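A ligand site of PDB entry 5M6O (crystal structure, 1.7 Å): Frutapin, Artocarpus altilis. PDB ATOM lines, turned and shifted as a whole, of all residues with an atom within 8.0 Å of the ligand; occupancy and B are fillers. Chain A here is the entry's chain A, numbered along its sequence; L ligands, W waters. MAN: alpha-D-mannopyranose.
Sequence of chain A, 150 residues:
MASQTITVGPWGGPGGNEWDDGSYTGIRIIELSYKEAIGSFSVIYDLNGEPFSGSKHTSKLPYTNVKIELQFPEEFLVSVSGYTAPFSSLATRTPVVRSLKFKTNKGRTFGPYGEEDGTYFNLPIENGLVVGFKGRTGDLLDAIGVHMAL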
ATOM      1  N   GLY A  13      28.143  20.118 -28.398  1.00  0.00           N
ATOM      2  CA  GLY A  13      29.531  19.870 -28.035  1.00  0.00           C
ATOM      3  C   GLY A  13      29.754  18.993 -26.891  1.00  0.00           C
ATOM      4  O   GLY A  13      28.830  18.451 -26.359  1.00  0.00           O
ATOM      5  N   PRO A  14      31.001  18.792 -26.515  1.00  0.00           N
ATOM      6  CA  PRO A  14      31.437  17.820 -25.547  1.00  0.00           C
ATOM      7  C   PRO A  14      31.519  18.276 -24.158  1.00  0.00           C
ATOM      8  O   PRO A  14      32.001  17.523 -23.322  1.00  0.00           O
ATOM      9  CB  PRO A  14      32.871  17.495 -26.028  1.00  0.00           C
ATOM     10  CG  PRO A  14      33.340  18.734 -26.588  1.00  0.00           C
ATOM     11  CD  PRO A  14      32.145  19.319 -27.306  1.00  0.00           C
ATOM     12  N   GLY A  15      31.072  19.505 -23.881  1.00  0.00           N
ATOM     13  CA  GLY A  15      31.039  20.048 -22.558  1.00  0.00           C
ATOM     14  C   GLY A  15      29.901  19.481 -21.682  1.00  0.00           C
ATOM     15  O   GLY A  15      29.052  18.715 -22.075  1.00  0.00           O
ATOM     16  N   GLY A  16      29.886  19.952 -20.473  1.00  0.00           N
ATOM     17  CA  GLY A  16      28.902  19.558 -19.507  1.00  0.00           C
ATOM     18  C   GLY A  16      29.013  18.072 -19.171  1.00  0.00           C
ATOM     19  O   GLY A  16      30.062  17.470 -19.317  1.00  0.00           O
ATOM     20  N   ASN A  17      27.936  17.538 -18.628  1.00  0.00           N
ATOM     21  CA  ASN A  17      27.846  16.130 -18.182  1.00  0.00           C
ATOM     22  C   ASN A  17      26.732  15.428 -18.917  1.00  0.00           C
ATOM     23  O   ASN A  17      25.611  15.987 -19.036  1.00  0.00           O
ATOM     24  CB  ASN A  17      27.569  16.142 -16.714  1.00  0.00           C
ATOM     25  CG  ASN A  17      28.786  16.602 -15.897  1.00  0.00           C
ATOM     26  OD1 ASN A  17      29.810  15.959 -15.964  1.00  0.00           O
ATOM     27  ND2 ASN A  17      28.634  17.636 -15.114  1.00  0.00           N
ATOM     28  N   ILE A  38      19.994  27.514 -24.745  1.00  0.00           N
ATOM     29  CA  ILE A  38      19.013  26.667 -23.986  1.00  0.00           C
ATOM     30  C   ILE A  38      19.694  26.318 -22.671  1.00  0.00           C
ATOM     31  O   ILE A  38      20.858  25.931 -22.651  1.00  0.00           O
ATOM     32  CB  ILE A  38      18.706  25.434 -24.815  1.00  0.00           C
ATOM     33  CG1 ILE A  38      18.127  25.671 -26.166  1.00  0.00           C
ATOM     34  CG2 ILE A  38      17.714  24.545 -24.069  1.00  0.00           C
ATOM     35  CD1 ILE A  38      16.812  26.434 -26.123  1.00  0.00           C
ATOM     36  N   GLY A  39      18.963  26.428 -21.568  1.00  0.00           N
ATOM     37  CA  GLY A  39      19.413  26.109 -20.284  1.00  0.00           C
ATOM     38  C   GLY A  39      18.916  24.774 -19.778  1.00  0.00           C
ATOM     39  O   GLY A  39      19.522  23.702 -20.044  1.00  0.00           O
ATOM     40  N   SER A  59      19.178  23.992 -15.465  1.00  0.00           N
ATOM     41  CA  SER A  59      20.110  25.151 -15.358  1.00  0.00           C
ATOM     42  C   SER A  59      19.649  26.077 -14.228  1.00  0.00           C
ATOM     43  O   SER A  59      18.483  26.547 -14.216  1.00  0.00           O
ATOM     44  CB  SER A  59      20.169  25.982 -16.626  1.00  0.00           C
ATOM     45  OG  SER A  59      21.024  27.128 -16.457  1.00  0.00           O
ATOM     46  N   LEU A  61      20.844  29.139 -14.116  1.00  0.00           N
ATOM     47  CA  LEU A  61      20.784  30.475 -14.739  1.00  0.00           C
ATOM     48  C   LEU A  61      19.326  30.978 -14.814  1.00  0.00           C
ATOM     49  O   LEU A  61      18.399  30.184 -15.120  1.00  0.00           O
ATOM     50  CB  LEU A  61      21.335  30.394 -16.179  1.00  0.00           C
ATOM     51  CG  LEU A  61      22.798  29.997 -16.341  1.00  0.00           C
ATOM     52  CD1 LEU A  61      23.175  29.923 -17.816  1.00  0.00           C
ATOM     53  CD2 LEU A  61      23.725  30.942 -15.580  1.00  0.00           C
ATOM     54  N   PHE A  87      29.065  29.994 -26.692  1.00  0.00           N
ATOM     55  CA  PHE A  87      28.383  31.095 -26.081  1.00  0.00           C
ATOM     56  C   PHE A  87      29.394  31.775 -25.161  1.00  0.00           C
ATOM     57  O   PHE A  87      29.894  31.167 -24.212  1.00  0.00           O
ATOM     58  CB  PHE A  87      27.041  30.627 -25.448  1.00  0.00           C
ATOM     59  CG  PHE A  87      26.321  31.691 -24.708  1.00  0.00           C
ATOM     60  CD1 PHE A  87      26.048  32.942 -25.297  1.00  0.00           C
ATOM     61  CD2 PHE A  87      25.930  31.473 -23.422  1.00  0.00           C
ATOM     62  CE1 PHE A  87      25.430  33.940 -24.573  1.00  0.00           C
ATOM     63  CE2 PHE A  87      25.323  32.447 -22.690  1.00  0.00           C
ATOM     64  CZ  PHE A  87      25.061  33.687 -23.253  1.00  0.00           C
ATOM     65  N   SER A  89      30.744  33.685 -22.479  1.00  0.00           N
ATOM     66  CA  SER A  89      31.542  33.403 -21.264  1.00  0.00           C
ATOM     67  C   SER A  89      31.380  31.986 -20.725  1.00  0.00           C
ATOM     68  O   SER A  89      32.359  31.339 -20.326  1.00  0.00           O
ATOM     69  CB  SER A  89      31.256  34.409 -20.152  1.00  0.00           C
ATOM     70  OG  SER A  89      32.391  35.230 -19.971  1.00  0.00           O
ATOM     71  N   LEU A  90      30.148  31.509 -20.731  1.00  0.00           N
ATOM     72  CA  LEU A  90      29.832  30.227 -20.142  1.00  0.00           C
ATOM     73  C   LEU A  90      30.343  29.022 -20.969  1.00  0.00           C
ATOM     74  O   LEU A  90      30.625  27.984 -20.391  1.00  0.00           O
ATOM     75  CB  LEU A  90      28.323  30.100 -19.903  1.00  0.00           C
ATOM     76  CG  LEU A  90      27.817  30.804 -18.650  1.00  0.00           C
ATOM     77  CD1 LEU A  90      28.062  32.305 -18.680  1.00  0.00           C
ATOM     78  CD2 LEU A  90      26.338  30.519 -18.554  1.00  0.00           C
ATOM     79  N   ALA A  91      30.444  29.162 -22.290  1.00  0.00           N
ATOM     80  CA  ALA A  91      30.824  28.055 -23.157  1.00  0.00           C
ATOM     81  C   ALA A  91      31.731  28.578 -24.235  1.00  0.00           C
ATOM     82  O   ALA A  91      31.335  28.687 -25.422  1.00  0.00           O
ATOM     83  CB  ALA A  91      29.594  27.444 -23.759  1.00  0.00           C
ATOM     84  N   THR A  92      32.967  28.894 -23.859  1.00  0.00           N
ATOM     85  CA  THR A  92      33.868  29.528 -24.820  1.00  0.00           C
ATOM     86  C   THR A  92      34.556  28.536 -25.711  1.00  0.00           C
ATOM     87  O   THR A  92      34.917  28.898 -26.872  1.00  0.00           O
ATOM     88  CB  THR A  92      34.903  30.349 -24.090  1.00  0.00           C
ATOM     89  OG1 THR A  92      34.174  31.306 -23.292  1.00  0.00           O
ATOM     90  CG2 THR A  92      35.788  31.056 -25.103  1.00  0.00           C
ATOM     91  N   ARG A  93      34.770  27.319 -25.184  1.00  0.00           N
ATOM     92  CA  ARG A  93      35.532  26.387 -25.950  1.00  0.00           C
ATOM     93  C   ARG A  93      34.763  25.546 -26.877  1.00  0.00           C
ATOM     94  O   ARG A  93      35.279  25.254 -27.942  1.00  0.00           O
ATOM     95  CB  ARG A  93      36.357  25.486 -25.073  1.00  0.00           C
ATOM     96  CG  ARG A  93      37.364  26.209 -24.281  1.00  0.00           C
ATOM     97  CD  ARG A  93      38.253  25.196 -23.573  1.00  0.00           C
ATOM     98  NE  ARG A  93      39.416  25.941 -23.155  1.00  0.00           N
ATOM     99  CZ  ARG A  93      40.618  25.848 -23.699  1.00  0.00           C
ATOM    100  NH1 ARG A  93      40.896  24.948 -24.609  1.00  0.00           N
ATOM    101  NH2 ARG A  93      41.548  26.649 -23.237  1.00  0.00           N
ATOM    102  N   THR A  94      33.554  25.108 -26.447  1.00  0.00           N
ATOM    103  CA  THR A  94      32.835  24.127 -27.138  1.00  0.00           C
ATOM    104  C   THR A  94      31.435  24.683 -27.394  1.00  0.00           C
ATOM    105  O   THR A  94      31.022  25.589 -26.617  1.00  0.00           O
ATOM    106  CB  THR A  94      32.866  22.808 -26.314  1.00  0.00           C
ATOM    107  OG1 THR A  94      32.440  23.051 -24.967  1.00  0.00           O
ATOM    108  CG2 THR A  94      34.322  22.302 -26.313  1.00  0.00           C
ATOM    109  N   PRO A  95      30.805  24.238 -28.533  1.00  0.00           N
ATOM    110  CA  PRO A  95      29.466  24.631 -28.893  1.00  0.00           C
ATOM    111  C   PRO A  95      28.445  24.081 -27.904  1.00  0.00           C
ATOM    112  O   PRO A  95      28.660  22.984 -27.429  1.00  0.00           O
ATOM    113  CB  PRO A  95      29.233  24.000 -30.307  1.00  0.00           C
ATOM    114  CG  PRO A  95      30.435  23.209 -30.564  1.00  0.00           C
ATOM    115  CD  PRO A  95      31.503  23.783 -29.742  1.00  0.00           C
ATOM    116  N   VAL A  96      27.358  24.819 -27.695  1.00  0.00           N
ATOM    117  CA  VAL A  96      26.208  24.474 -26.817  1.00  0.00           C
ATOM    118  C   VAL A  96      25.041  24.632 -27.723  1.00  0.00           C
ATOM    119  O   VAL A  96      25.134  25.138 -28.846  1.00  0.00           O
ATOM    120  CB  VAL A  96      26.085  25.398 -25.568  1.00  0.00           C
ATOM    121  CG1 VAL A  96      27.356  25.211 -24.718  1.00  0.00           C
ATOM    122  CG2 VAL A  96      25.809  26.869 -25.921  1.00  0.00           C
ATOM    123  N   VAL A  97      23.885  24.173 -27.236  1.00  0.00           N
ATOM    124  CA  VAL A  97      22.649  24.280 -28.037  1.00  0.00           C
ATOM    125  C   VAL A  97      22.146  25.727 -27.765  1.00  0.00           C
ATOM    126  O   VAL A  97      21.830  26.064 -26.620  1.00  0.00           O
ATOM    127  CB  VAL A  97      21.638  23.256 -27.584  1.00  0.00           C
ATOM    128  CG1 VAL A  97      20.210  23.512 -28.219  1.00  0.00           C
ATOM    129  CG2 VAL A  97      22.200  21.896 -27.846  1.00  0.00           C
ATOM    130  N   ARG A 136      23.665  16.561 -22.975  1.00  0.00           N
ATOM    131  CA  ARG A 136      24.770  16.821 -22.001  1.00  0.00           C
ATOM    132  C   ARG A 136      24.380  18.176 -21.463  1.00  0.00           C
ATOM    133  O   ARG A 136      23.961  19.053 -22.256  1.00  0.00           O
ATOM    134  CB  ARG A 136      26.103  16.992 -22.726  1.00  0.00           C
ATOM    135  CG  ARG A 136      26.566  15.843 -23.588  1.00  0.00           C
ATOM    136  CD  ARG A 136      28.007  15.946 -24.159  1.00  0.00           C
ATOM    137  NE  ARG A 136      28.943  16.066 -23.065  1.00  0.00           N
ATOM    138  CZ  ARG A 136      29.576  15.075 -22.432  1.00  0.00           C
ATOM    139  NH1 ARG A 136      30.224  15.410 -21.376  1.00  0.00           N
ATOM    140  NH2 ARG A 136      29.290  13.760 -22.658  1.00  0.00           N
ATOM    141  N   THR A 137      24.584  18.357 -20.178  1.00  0.00           N
ATOM    142  CA  THR A 137      24.196  19.618 -19.605  1.00  0.00           C
ATOM    143  C   THR A 137      25.259  19.975 -18.558  1.00  0.00           C
ATOM    144  O   THR A 137      25.608  19.121 -17.722  1.00  0.00           O
ATOM    145  CB  THR A 137      22.880  19.576 -18.858  1.00  0.00           C
ATOM    146  OG1 THR A 137      21.770  19.233 -19.759  1.00  0.00           O
ATOM    147  CG2 THR A 137      22.625  20.966 -18.135  1.00  0.00           C
ATOM    148  N   GLY A 138      25.662  21.254 -18.563  1.00  0.00           N
ATOM    149  CA  GLY A 138      26.530  21.787 -17.506  1.00  0.00           C
ATOM    150  C   GLY A 138      25.744  22.899 -16.823  1.00  0.00           C
ATOM    151  O   GLY A 138      24.716  22.663 -16.212  1.00  0.00           O
ATOM    152  N   ASP A 139      26.161  24.164 -17.052  1.00  0.00           N
ATOM    153  CA  ASP A 139      25.277  25.339 -16.877  1.00  0.00           C
ATOM    154  C   ASP A 139      24.222  25.493 -17.918  1.00  0.00           C
ATOM    155  O   ASP A 139      23.209  26.172 -17.691  1.00  0.00           O
ATOM    156  CB  ASP A 139      26.091  26.663 -16.773  1.00  0.00           C
ATOM    157  CG  ASP A 139      27.107  26.656 -15.609  1.00  0.00           C
ATOM    158  OD1 ASP A 139      26.799  26.108 -14.516  1.00  0.00           O
ATOM    159  OD2 ASP A 139      28.219  27.213 -15.784  1.00  0.00           O
ATOM    160  N   LEU A 140      24.441  24.904 -19.100  1.00  0.00           N
ATOM    161  CA  LEU A 140      23.565  25.030 -20.267  1.00  0.00           C
ATOM    162  C   LEU A 140      23.397  23.664 -20.931  1.00  0.00           C
ATOM    163  O   LEU A 140      24.111  22.716 -20.536  1.00  0.00           O
ATOM    164  CB  LEU A 140      24.258  25.892 -21.380  1.00  0.00           C
ATOM    165  CG  LEU A 140      24.518  27.395 -21.071  1.00  0.00           C
ATOM    166  CD1 LEU A 140      25.239  28.007 -22.239  1.00  0.00           C
ATOM    167  CD2 LEU A 140      23.191  28.076 -20.852  1.00  0.00           C
ATOM    168  N   LEU A 141      22.439  23.550 -21.862  1.00  0.00           N
ATOM    169  CA  LEU A 141      22.355  22.341 -22.677  1.00  0.00           C
ATOM    170  C   LEU A 141      23.487  22.363 -23.685  1.00  0.00           C
ATOM    171  O   LEU A 141      23.395  23.114 -24.708  1.00  0.00           O
ATOM    172  CB  LEU A 141      21.043  22.368 -23.419  1.00  0.00           C
ATOM    173  CG  LEU A 141      20.661  21.162 -24.260  1.00  0.00           C
ATOM    174  CD1 LEU A 141      20.611  20.000 -23.345  1.00  0.00           C
ATOM    175  CD2 LEU A 141      19.320  21.374 -24.950  1.00  0.00           C
ATOM    176  N   ASP A 142      24.583  21.621 -23.428  1.00  0.00           N
ATOM    177  CA  ASP A 142      25.671  21.475 -24.327  1.00  0.00           C
ATOM    178  C   ASP A 142      25.328  20.657 -25.577  1.00  0.00           C
ATOM    179  O   ASP A 142      25.843  20.916 -26.671  1.00  0.00           O
ATOM    180  CB  ASP A 142      26.853  20.803 -23.631  1.00  0.00           C
ATOM    181  CG  ASP A 142      27.517  21.681 -22.672  1.00  0.00           C
ATOM    182  OD1 ASP A 142      27.131  21.732 -21.508  1.00  0.00           O
ATOM    183  OD2 ASP A 142      28.513  22.330 -23.060  1.00  0.00           O
ATOM    184  N   ALA A 143      24.526  19.584 -25.419  1.00  0.00           N
ATOM    185  CA  ALA A 143      24.185  18.730 -26.565  1.00  0.00           C
ATOM    186  C   ALA A 143      22.809  18.140 -26.422  1.00  0.00           C
ATOM    187  O   ALA A 143      22.379  17.990 -25.267  1.00  0.00           O
ATOM    188  CB  ALA A 143      25.224  17.625 -26.855  1.00  0.00           C
HETATM  189  C1  MAN L   1      30.060  24.496 -17.538  1.00  0.00           C
HETATM  190  C2  MAN L   1      30.754  23.192 -17.810  1.00  0.00           C
HETATM  191  C3  MAN L   1      31.168  23.139 -19.273  1.00  0.00           C
HETATM  192  C4  MAN L   1      29.959  23.466 -20.179  1.00  0.00           C
HETATM  193  C5  MAN L   1      29.248  24.804 -19.761  1.00  0.00           C
HETATM  194  C6  MAN L   1      27.936  24.966 -20.538  1.00  0.00           C
HETATM  195  O1  MAN L   1      31.027  25.523 -17.831  1.00  0.00           O
HETATM  196  O2  MAN L   1      29.815  22.216 -17.241  1.00  0.00           O
HETATM  197  O3  MAN L   1      31.788  21.907 -19.547  1.00  0.00           O
HETATM  198  O4  MAN L   1      30.255  23.439 -21.576  1.00  0.00           O
HETATM  199  O5  MAN L   1      28.891  24.779 -18.362  1.00  0.00           O
HETATM  200  O6  MAN L   1      26.986  23.926 -20.164  1.00  0.00           O
HETATM  201  O   HOH W   1      29.659  27.556 -18.047  1.00  0.00           O
HETATM  202  O   HOH W   2      31.004  19.714 -15.592  1.00  0.00           O
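O5 of the ligand lies within hydrogen-bond range of N of Asp 139. O3 of the ligand lies within hydrogen-bond range of N of Gly 16, at 2.9 Å. The side-chain carboxylate of Asp 142 sits at hydrogen-bond distance from an oxygen (O4) of the ligand. The backbone carbonyl oxygen of Leu 140 lies within hydrogen-bond range of an oxygen (O6) of the ligand, 3.1 Å away. The backbone NH (N) of Gly 138 is in hydrogen-bond range of an oxygen (O6) of the ligand, 3.4 Å away. The backbone NH (N) of Leu 140 sits at hydrogen-bond distance from an oxygen (O6) of the ligand (2.9 Å).
The backbone carbonyl oxygen (O) of Asp 142 is in hydrogen-bond range of the backbone NH (N) of Gly 13, at 3.0 Å. The guanidinium group of Arg 136 is in hydrogen-bond range of the backbone carbonyl oxygen of Gly 15, 2.8 Å away. The guanidinium group of Arg 136 lies within hydrogen-bond range of the backbone carbonyl oxygen of Gly 16, at 2.9 Å. The backbone carbonyl oxygen (O) of Asp 139 sits at hydrogen-bond distance from the side-chain hydroxyl (OG) of Ser 59, at 2.7 Å. The side-chain carboxylate (OD1) of Asp 142 lies within hydrogen-bond range of the backbone NH (N) of Gly 138. The backbone NH (N) of Gly 16 sits at hydrogen-bond distance from the side-chain carboxylate (OD1) of Asp 142, at 3.4 Å. The backbone NH (N) of Asp 142 sits at hydrogen-bond distance from the backbone carbonyl oxygen (O) of Arg 136.
Gly 15 touches the ligand (CA to O4, 3.6 Å). Leu 90 touches the ligand. Hydrophobic or aromatic side chains within 4 Å of the ligand: Leu 140.
Water W1 lies within hydrogen-bond range of O1 of the ligand (2.5 Å), O of Leu 90 (2.6 Å) and OD2 of Asp 139 (2.7 Å). Water W2 lies within hydrogen-bond range of ND2 of Asn 17 and O2 of the ligand.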
